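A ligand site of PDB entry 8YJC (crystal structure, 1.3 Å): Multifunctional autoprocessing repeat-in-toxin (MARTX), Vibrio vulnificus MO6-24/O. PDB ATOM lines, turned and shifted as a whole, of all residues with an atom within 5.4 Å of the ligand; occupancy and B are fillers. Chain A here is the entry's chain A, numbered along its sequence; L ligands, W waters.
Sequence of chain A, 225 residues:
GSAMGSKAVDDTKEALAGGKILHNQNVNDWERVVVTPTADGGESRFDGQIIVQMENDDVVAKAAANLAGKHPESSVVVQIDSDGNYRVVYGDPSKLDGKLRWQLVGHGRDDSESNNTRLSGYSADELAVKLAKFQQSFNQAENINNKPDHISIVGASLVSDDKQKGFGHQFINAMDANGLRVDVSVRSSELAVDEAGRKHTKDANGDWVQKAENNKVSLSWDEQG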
ATOM      1  N   GLY A  41      32.119  23.173 -20.301  1.00  0.00           N
ATOM      2  CA  GLY A  41      31.006  22.336 -20.713  1.00  0.00           C
ATOM      3  C   GLY A  41      31.365  21.215 -21.665  1.00  0.00           C
ATOM      4  O   GLY A  41      30.571  20.282 -21.834  1.00  0.00           O
ATOM      5  N   GLU A  43      32.169  19.117 -25.215  1.00  0.00           N
ATOM      6  CA  GLU A  43      31.499  18.982 -26.500  1.00  0.00           C
ATOM      7  C   GLU A  43      30.116  18.389 -26.316  1.00  0.00           C
ATOM      8  O   GLU A  43      29.865  17.602 -25.394  1.00  0.00           O
ATOM      9  CB  GLU A  43      32.307  18.122 -27.465  1.00  0.00           C
ATOM     10  CG  GLU A  43      33.426  18.871 -28.197  1.00  0.00           C
ATOM     11  CD  GLU A  43      34.571  17.970 -28.587  1.00  0.00           C
ATOM     12  OE1 GLU A  43      34.433  16.732 -28.486  1.00  0.00           O
ATOM     13  OE2 GLU A  43      35.630  18.506 -29.013  1.00  0.00           O
ATOM     14  N   SER A  44      29.205  18.772 -27.203  1.00  0.00           N
ATOM     15  CA  SER A  44      27.848  18.260 -27.216  1.00  0.00           C
ATOM     16  C   SER A  44      27.565  17.719 -28.601  1.00  0.00           C
ATOM     17  O   SER A  44      28.063  18.252 -29.598  1.00  0.00           O
ATOM     18  CB  SER A  44      26.872  19.394 -26.880  1.00  0.00           C
ATOM     19  OG  SER A  44      25.526  18.950 -26.879  1.00  0.00           O
ATOM     20  N   ARG A  45      26.794  16.631 -28.681  1.00  0.00           N
ATOM     21  CA  ARG A  45      26.411  16.158 -30.000  1.00  0.00           C
ATOM     22  C   ARG A  45      25.399  17.082 -30.672  1.00  0.00           C
ATOM     23  O   ARG A  45      25.159  16.940 -31.874  1.00  0.00           O
ATOM     24  CB  ARG A  45      25.905  14.717 -29.962  1.00  0.00           C
ATOM     25  CG  ARG A  45      24.630  14.533 -29.189  1.00  0.00           C
ATOM     26  CD  ARG A  45      24.104  13.095 -29.289  1.00  0.00           C
ATOM     27  NE  ARG A  45      23.171  12.836 -28.209  1.00  0.00           N
ATOM     28  CZ  ARG A  45      22.051  12.134 -28.314  1.00  0.00           C
ATOM     29  NH1 ARG A  45      21.702  11.539 -29.443  1.00  0.00           N
ATOM     30  NH2 ARG A  45      21.228  12.057 -27.257  1.00  0.00           N
ATOM     31  N   PHE A  46      24.836  18.038 -29.942  1.00  0.00           N
ATOM     32  CA  PHE A  46      23.810  18.914 -30.478  1.00  0.00           C
ATOM     33  C   PHE A  46      24.422  20.208 -30.956  1.00  0.00           C
ATOM     34  O   PHE A  46      25.213  20.828 -30.250  1.00  0.00           O
ATOM     35  CB  PHE A  46      22.732  19.138 -29.404  1.00  0.00           C
ATOM     36  CG  PHE A  46      22.055  17.875 -29.018  1.00  0.00           C
ATOM     37  CD1 PHE A  46      21.172  17.266 -29.893  1.00  0.00           C
ATOM     38  CD2 PHE A  46      22.348  17.237 -27.819  1.00  0.00           C
ATOM     39  CE1 PHE A  46      20.574  16.072 -29.573  1.00  0.00           C
ATOM     40  CE2 PHE A  46      21.753  16.031 -27.487  1.00  0.00           C
ATOM     41  CZ  PHE A  46      20.867  15.454 -28.364  1.00  0.00           C
ATOM     42  N   LYS A  70      26.041  26.015 -19.619  1.00  0.00           N
ATOM     43  CA  LYS A  70      26.989  24.970 -19.969  1.00  0.00           C
ATOM     44  C   LYS A  70      27.399  25.063 -21.436  1.00  0.00           C
ATOM     45  O   LYS A  70      28.525  24.687 -21.792  1.00  0.00           O
ATOM     46  CB  LYS A  70      26.391  23.593 -19.677  1.00  0.00           C
ATOM     47  CG  LYS A  70      27.423  22.471 -19.773  1.00  0.00           C
ATOM     48  CD  LYS A  70      26.835  21.089 -19.586  1.00  0.00           C
ATOM     49  CE  LYS A  70      27.941  20.045 -19.707  1.00  0.00           C
ATOM     50  NZ  LYS A  70      27.397  18.691 -19.925  1.00  0.00           N
ATOM     51  N   HIS A  71      26.501  25.524 -22.309  1.00  0.00           N
ATOM     52  CA  HIS A  71      26.775  25.674 -23.738  1.00  0.00           C
ATOM     53  C   HIS A  71      26.313  27.065 -24.147  1.00  0.00           C
ATOM     54  O   HIS A  71      25.322  27.229 -24.868  1.00  0.00           O
ATOM     55  CB  HIS A  71      26.101  24.564 -24.557  1.00  0.00           C
ATOM     56  CG  HIS A  71      26.548  23.199 -24.176  1.00  0.00           C
ATOM     57  ND1 HIS A  71      27.846  22.754 -24.372  1.00  0.00           N
ATOM     58  CD2 HIS A  71      25.907  22.188 -23.543  1.00  0.00           C
ATOM     59  CE1 HIS A  71      27.967  21.526 -23.903  1.00  0.00           C
ATOM     60  NE2 HIS A  71      26.804  21.161 -23.394  1.00  0.00           N
ATOM     61  N   ARG A 101      18.548  19.640 -29.515  1.00  0.00           N
ATOM     62  CA  ARG A 101      17.931  19.099 -28.319  1.00  0.00           C
ATOM     63  C   ARG A 101      17.009  20.151 -27.709  1.00  0.00           C
ATOM     64  O   ARG A 101      17.284  21.358 -27.784  1.00  0.00           O
ATOM     65  CB  ARG A 101      19.023  18.709 -27.312  1.00  0.00           C
ATOM     66  CG  ARG A 101      18.518  18.344 -25.910  1.00  0.00           C
ATOM     67  CD  ARG A 101      19.627  17.774 -25.022  1.00  0.00           C
ATOM     68  NE  ARG A 101      20.717  18.727 -24.882  1.00  0.00           N
ATOM     69  CZ  ARG A 101      21.941  18.409 -24.461  1.00  0.00           C
ATOM     70  NH1 ARG A 101      22.228  17.199 -24.032  1.00  0.00           N
ATOM     71  NH2 ARG A 101      22.877  19.354 -24.461  1.00  0.00           N
ATOM     72  N   GLN A 103      15.744  20.714 -23.784  1.00  0.00           N
ATOM     73  CA  GLN A 103      15.744  20.270 -22.387  1.00  0.00           C
ATOM     74  C   GLN A 103      14.557  20.933 -21.694  1.00  0.00           C
ATOM     75  O   GLN A 103      14.499  22.162 -21.627  1.00  0.00           O
ATOM     76  CB  GLN A 103      17.057  20.612 -21.684  1.00  0.00           C
ATOM     77  CG  GLN A 103      18.279  20.140 -22.453  1.00  0.00           C
ATOM     78  CD  GLN A 103      19.464  19.829 -21.539  1.00  0.00           C
ATOM     79  OE1 GLN A 103      19.320  19.145 -20.521  1.00  0.00           O
ATOM     80  NE2 GLN A 103      20.647  20.324 -21.913  1.00  0.00           N
ATOM     81  N   HIS A 150      15.987  15.314 -30.073  1.00  0.00           N
ATOM     82  CA  HIS A 150      16.057  14.706 -28.751  1.00  0.00           C
ATOM     83  C   HIS A 150      15.443  15.642 -27.727  1.00  0.00           C
ATOM     84  O   HIS A 150      15.718  16.844 -27.727  1.00  0.00           O
ATOM     85  CB  HIS A 150      17.516  14.453 -28.374  1.00  0.00           C
ATOM     86  CG  HIS A 150      17.659  13.689 -27.105  1.00  0.00           C
ATOM     87  ND1 HIS A 150      17.686  12.307 -27.083  1.00  0.00           N
ATOM     88  CD2 HIS A 150      17.704  14.094 -25.816  1.00  0.00           C
ATOM     89  CE1 HIS A 150      17.776  11.904 -25.822  1.00  0.00           C
ATOM     90  NE2 HIS A 150      17.774  12.969 -25.035  1.00  0.00           N
ATOM     91  N   SER A 152      15.360  16.026 -23.620  1.00  0.00           N
ATOM     92  CA  SER A 152      15.813  15.641 -22.284  1.00  0.00           C
ATOM     93  C   SER A 152      14.805  16.192 -21.265  1.00  0.00           C
ATOM     94  O   SER A 152      14.617  17.408 -21.187  1.00  0.00           O
ATOM     95  CB  SER A 152      17.210  16.170 -22.038  1.00  0.00           C
ATOM     96  OG  SER A 152      17.662  15.798 -20.746  1.00  0.00           O
ATOM     97  N   SER A 185      15.111  11.307 -23.268  1.00  0.00           N
ATOM     98  CA  SER A 185      15.794  10.860 -22.063  1.00  0.00           C
ATOM     99  C   SER A 185      15.052  11.359 -20.834  1.00  0.00           C
ATOM    100  O   SER A 185      14.531  12.477 -20.817  1.00  0.00           O
ATOM    101  CB  SER A 185      17.274  11.264 -22.061  1.00  0.00           C
ATOM    102  OG  SER A 185      17.443  12.662 -22.196  1.00  0.00           O
ATOM    103  N   ARG A 187      14.315  10.512 -16.299  1.00  0.00           N
ATOM    104  CA  ARG A 187      14.899   9.983 -15.067  1.00  0.00           C
ATOM    105  C   ARG A 187      13.829   9.436 -14.147  1.00  0.00           C
ATOM    106  O   ARG A 187      12.734  10.007 -14.042  1.00  0.00           O
ATOM    107  CB  ARG A 187      15.683  11.074 -14.332  1.00  0.00           C
ATOM    108  CG  ARG A 187      16.952  11.532 -15.037  1.00  0.00           C
ATOM    109  CD  ARG A 187      16.682  12.607 -16.085  1.00  0.00           C
ATOM    110  NE  ARG A 187      17.937  13.050 -16.688  1.00  0.00           N
ATOM    111  CZ  ARG A 187      18.028  13.684 -17.846  1.00  0.00           C
ATOM    112  NH1 ARG A 187      16.958  14.027 -18.539  1.00  0.00           N
ATOM    113  NH2 ARG A 187      19.230  13.968 -18.337  1.00  0.00           N
ATOM    114  N   GLY A 197      25.555  23.590 -14.704  1.00  0.00           N
ATOM    115  CA  GLY A 197      24.617  23.030 -15.657  1.00  0.00           C
ATOM    116  C   GLY A 197      24.632  21.525 -15.757  1.00  0.00           C
ATOM    117  O   GLY A 197      24.104  20.978 -16.724  1.00  0.00           O
ATOM    118  N   ARG A 198      25.231  20.835 -14.787  1.00  0.00           N
ATOM    119  CA  ARG A 198      25.291  19.375 -14.783  1.00  0.00           C
ATOM    120  C   ARG A 198      24.202  18.813 -13.880  1.00  0.00           C
ATOM    121  O   ARG A 198      23.853  19.394 -12.847  1.00  0.00           O
ATOM    122  CB  ARG A 198      26.675  18.878 -14.345  1.00  0.00           C
ATOM    123  CG  ARG A 198      27.778  19.308 -15.304  1.00  0.00           C
ATOM    124  CD  ARG A 198      29.108  18.608 -15.014  1.00  0.00           C
ATOM    125  NE  ARG A 198      30.123  18.995 -15.976  1.00  0.00           N
ATOM    126  CZ  ARG A 198      30.319  18.385 -17.137  1.00  0.00           C
ATOM    127  NH1 ARG A 198      29.616  17.322 -17.493  1.00  0.00           N
ATOM    128  NH2 ARG A 198      31.253  18.843 -17.972  1.00  0.00           N
ATOM    129  N   LYS A 199      23.692  17.659 -14.272  1.00  0.00           N
ATOM    130  CA  LYS A 199      22.593  17.031 -13.568  1.00  0.00           C
ATOM    131  C   LYS A 199      23.102  16.076 -12.488  1.00  0.00           C
ATOM    132  O   LYS A 199      24.146  15.446 -12.612  1.00  0.00           O
ATOM    133  CB  LYS A 199      21.721  16.263 -14.564  1.00  0.00           C
ATOM    134  CG  LYS A 199      21.280  17.158 -15.734  1.00  0.00           C
ATOM    135  CD  LYS A 199      20.381  16.447 -16.711  1.00  0.00           C
ATOM    136  CE  LYS A 199      19.981  17.362 -17.863  1.00  0.00           C
ATOM    137  NZ  LYS A 199      20.987  17.554 -18.943  1.00  0.00           N
ATOM    138  N   GLN A 210      26.334  12.005  -9.506  1.00  0.00           N
ATOM    139  CA  GLN A 210      26.404  12.373 -10.905  1.00  0.00           C
ATOM    140  C   GLN A 210      26.741  11.157 -11.755  1.00  0.00           C
ATOM    141  O   GLN A 210      27.479  10.259 -11.340  1.00  0.00           O
ATOM    142  CB  GLN A 210      27.461  13.450 -11.139  1.00  0.00           C
ATOM    143  CG  GLN A 210      27.105  14.789 -10.516  1.00  0.00           C
ATOM    144  CD  GLN A 210      28.213  15.798 -10.673  1.00  0.00           C
ATOM    145  OE1 GLN A 210      28.448  16.334 -11.758  1.00  0.00           O
ATOM    146  NE2 GLN A 210      28.925  16.071  -9.591  1.00  0.00           N
ATOM    147  N   LYS A 211      26.196  11.154 -12.969  1.00  0.00           N
ATOM    148  CA  LYS A 211      26.494  10.132 -13.981  1.00  0.00           C
ATOM    149  C   LYS A 211      26.060   8.739 -13.534  1.00  0.00           C
ATOM    150  O   LYS A 211      26.680   7.736 -13.902  1.00  0.00           O
ATOM    151  CB  LYS A 211      27.941  10.188 -14.473  1.00  0.00           C
ATOM    152  CG  LYS A 211      28.308  11.553 -15.067  1.00  0.00           C
ATOM    153  CD  LYS A 211      27.290  11.993 -16.141  1.00  0.00           C
ATOM    154  CE  LYS A 211      27.891  12.576 -17.432  1.00  0.00           C
ATOM    155  NZ  LYS A 211      28.709  13.823 -17.292  1.00  0.00           N
ATOM    156  N   GLU A 213      24.000   6.327 -14.577  1.00  0.00           N
ATOM    157  CA  GLU A 213      23.214   5.932 -15.741  1.00  0.00           C
ATOM    158  C   GLU A 213      22.008   5.093 -15.358  1.00  0.00           C
ATOM    159  O   GLU A 213      20.989   5.118 -16.066  1.00  0.00           O
ATOM    160  CB  GLU A 213      24.114   5.220 -16.758  1.00  0.00           C
ATOM    161  CG  GLU A 213      25.273   6.058 -17.269  1.00  0.00           C
ATOM    162  CD  GLU A 213      24.786   7.123 -18.234  1.00  0.00           C
ATOM    163  OE1 GLU A 213      24.175   6.741 -19.250  1.00  0.00           O
ATOM    164  OE2 GLU A 213      25.006   8.319 -17.974  1.00  0.00           O
ATOM    165  N   LYS A 216      18.490   6.828 -15.371  1.00  0.00           N
ATOM    166  CA  LYS A 216      17.963   7.446 -16.580  1.00  0.00           C
ATOM    167  C   LYS A 216      17.754   6.364 -17.640  1.00  0.00           C
ATOM    168  O   LYS A 216      18.378   5.302 -17.604  1.00  0.00           O
ATOM    169  CB  LYS A 216      18.935   8.512 -17.121  1.00  0.00           C
ATOM    170  CG  LYS A 216      18.382   9.387 -18.250  1.00  0.00           C
ATOM    171  CD  LYS A 216      19.347  10.513 -18.609  1.00  0.00           C
ATOM    172  CE  LYS A 216      20.439  10.039 -19.519  1.00  0.00           C
ATOM    173  NZ  LYS A 216      21.364  11.135 -19.906  1.00  0.00           N
HETATM  174  C1  LIG L   1      26.237  15.039 -20.715  1.00  0.00           C
HETATM  175  C2  LIG L   1      25.630  15.256 -22.101  1.00  0.00           C
HETATM  176  C3  LIG L   1      24.386  14.366 -22.209  1.00  0.00           C
HETATM  177  C4  LIG L   1      23.361  14.659 -21.116  1.00  0.00           C
HETATM  178  C5  LIG L   1      24.041  14.347 -19.773  1.00  0.00           C
HETATM  179  C6  LIG L   1      25.226  15.308 -19.615  1.00  0.00           C
HETATM  180  O1  LIG L   1      27.320  15.929 -20.543  1.00  0.00           O
HETATM  181  P1  LIG L   1      28.853  15.382 -20.748  1.00  0.00           P
HETATM  182  O2  LIG L   1      29.641  16.528 -20.228  1.00  0.00           O
HETATM  183  O3  LIG L   1      29.062  15.140 -22.226  1.00  0.00           O
HETATM  184  O4  LIG L   1      29.019  14.094 -19.998  1.00  0.00           O
HETATM  185  O5  LIG L   1      25.207  16.589 -22.243  1.00  0.00           O
HETATM  186  P2  LIG L   1      26.003  17.667 -23.150  1.00  0.00           P
HETATM  187  O6  LIG L   1      25.951  18.927 -22.344  1.00  0.00           O
HETATM  188  O7  LIG L   1      27.425  17.179 -23.401  1.00  0.00           O
HETATM  189  O8  LIG L   1      25.225  17.823 -24.432  1.00  0.00           O
HETATM  190  O9  LIG L   1      23.791  14.584 -23.492  1.00  0.00           O
HETATM  191  P3  LIG L   1      23.445  13.312 -24.496  1.00  0.00           P
HETATM  192  O10 LIG L   1      21.947  13.391 -24.755  1.00  0.00           O
HETATM  193  O11 LIG L   1      23.824  12.005 -23.842  1.00  0.00           O
HETATM  194  O12 LIG L   1      24.196  13.503 -25.791  1.00  0.00           O
HETATM  195  O13 LIG L   1      22.281  13.777 -21.264  1.00  0.00           O
HETATM  196  P4  LIG L   1      20.746  14.311 -21.614  1.00  0.00           P
HETATM  197  O14 LIG L   1      20.747  14.820 -23.056  1.00  0.00           O
HETATM  198  O15 LIG L   1      19.923  13.045 -21.462  1.00  0.00           O
HETATM  199  O16 LIG L   1      20.374  15.415 -20.667  1.00  0.00           O
HETATM  200  O17 LIG L   1      23.131  14.505 -18.715  1.00  0.00           O
HETATM  201  P5  LIG L   1      23.024  13.341 -17.563  1.00  0.00           P
HETATM  202  O18 LIG L   1      23.596  12.075 -18.129  1.00  0.00           O
HETATM  203  O19 LIG L   1      23.802  13.817 -16.360  1.00  0.00           O
HETATM  204  O20 LIG L   1      21.575  13.245 -17.222  1.00  0.00           O
HETATM  205  O21 LIG L   1      25.852  15.056 -18.373  1.00  0.00           O
HETATM  206  P6  LIG L   1      25.965  16.247 -17.258  1.00  0.00           P
HETATM  207  O22 LIG L   1      24.793  16.061 -16.334  1.00  0.00           O
HETATM  208  O23 LIG L   1      27.274  16.003 -16.522  1.00  0.00           O
HETATM  209  O24 LIG L   1      25.897  17.600 -17.913  1.00  0.00           O
HETATM  210  O   HOH W   1      29.799  12.493 -22.779  1.00  0.00           O
HETATM  211  O   HOH W   2      24.077   9.863 -25.140  1.00  0.00           O
HETATM  212  O   HOH W   3      25.436  10.808 -19.587  1.00  0.00           O
HETATM  213  O   HOH W   4      25.851  15.611 -26.049  1.00  0.00           O
HETATM  214  O   HOH W   5      27.721  11.611 -20.938  1.00  0.00           O
HETATM  215  O   HOH W   6      23.470  19.608 -20.924  1.00  0.00           O
HETATM  216  O   HOH W   7      23.848  10.009 -16.329  1.00  0.00           O
HETATM  217  O   HOH W   8      26.649  11.903 -23.734  1.00  0.00           O
HETATM  218  O   HOH W   9      23.514  18.834 -18.297  1.00  0.00           O
HETATM  219  O   HOH W  10      30.350  17.692 -22.408  1.00  0.00           O
HETATM  220  O   HOH W  11      23.538  10.469 -21.617  1.00  0.00           O
HETATM  221  O   HOH W  12      26.780  15.314 -13.862  1.00  0.00           O
HETATM  222  O   HOH W  13      32.410  16.607 -20.331  1.00  0.00           O
HETATM  223  O   HOH W  14      20.228  12.392 -15.142  1.00  0.00           O
HETATM  224  O   HOH W  15      24.111  12.956 -13.751  1.00  0.00           O
HETATM  225  O   HOH W  16      26.239  11.765 -26.557  1.00  0.00           O
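O15 of the ligand is in salt-bridge range of NZ of Lys 216 (2.9 Å). NH2 of Arg 101 is in salt-bridge range of O8 of the ligand, at 2.8 Å. An oxygen (O8) of the ligand is in hydrogen-bond range of the side-chain hydroxyl (OG) of Ser 44, at 2.7 Å. A ring nitrogen (NE2) of His 71 lies within hydrogen-bond range of an oxygen (O6) of the ligand, at 2.6 Å. O12 of the ligand is in salt-bridge range of NE of Arg 45, at 2.7 Å. O23 of the ligand is in salt-bridge range of NZ of Lys 211, 2.7 Å away. O16 of the ligand sits at hydrogen-bond distance from OG of Ser 152 (2.7 Å). The side-chain amino group (NZ) of Lys 199 lies within salt-bridge range of an oxygen (O16) of the ligand (2.8 Å). The side-chain hydroxyl of Ser 185 sits at hydrogen-bond distance from an oxygen (O15) of the ligand (2.6 Å). An oxygen (O2) of the ligand lies within salt-bridge range of the guanidinium group (NH1) of Arg 198 (2.8 Å). An oxygen (O22) of the ligand lies within hydrogen-bond range of the backbone NH (N) of Lys 199. An oxygen (O24) of the ligand is in salt-bridge range of the side-chain amino group (NZ) of Lys 70 (2.7 Å). The guanidinium group of Arg 187 lies within salt-bridge range of an oxygen (O20) of the ligand (2.7 Å).
The side-chain amino group (NZ) of Lys 199 is in hydrogen-bond range of the side-chain amide oxygen (OE1) of Gln 103 (2.8 Å). The side-chain hydroxyl (OG) of Ser 44 sits close to the backbone NH (N) of Phe 46. The side-chain hydroxyl (OG) of Ser 185 sits close to the side-chain hydroxyl (OG) of Ser 152, 3.5 Å away. NE2 of His 150 lies within hydrogen-bond range of OG of Ser 185, at 2.9 Å. NE of Arg 101 sits close to NE2 of Gln 103, 3.4 Å away. The guanidinium group (NH1) of Arg 187 is in hydrogen-bond range of the side-chain hydroxyl (OG) of Ser 152 (2.9 Å).
The backbone carbonyl oxygen (O) of Glu 43 lies close to an oxygen (O7) of the ligand (3.2 Å). Phe 46 touches the ligand (CE2 to O10, 3.8 Å). Gln 103 touches the ligand. The nearest printed residue that does not touch the ligand is Gly 197 (4.005 Å).
Water W10 lies within hydrogen-bond range of an oxygen (O2) of the ligand (2.6 Å), the backbone carbonyl oxygen of Gly 41 (2.7 Å) and the backbone carbonyl oxygen of Glu 43 (3.0 Å). Water W3 bridges O18 of the ligand and OE2 of Glu 213. Water W4 lies within hydrogen-bond range of an oxygen (O12) of the ligand, the backbone NH of Arg 45 and the side-chain hydroxyl of Ser 44. Water W15 lies within hydrogen-bond range of O of Lys 199, O19 of the ligand and N of Lys 211. Water W12 lies within hydrogen-bond range of an oxygen (O23) of the ligand (2.8 Å), the side-chain amide oxygen of Gln 210 (2.9 Å) and the backbone carbonyl oxygen of Lys 199 (2.9 Å). Water W6 bridges an oxygen (O6) of the ligand (2.9 Å) and the side-chain amide nitrogen of Gln 103 (3.1 Å).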
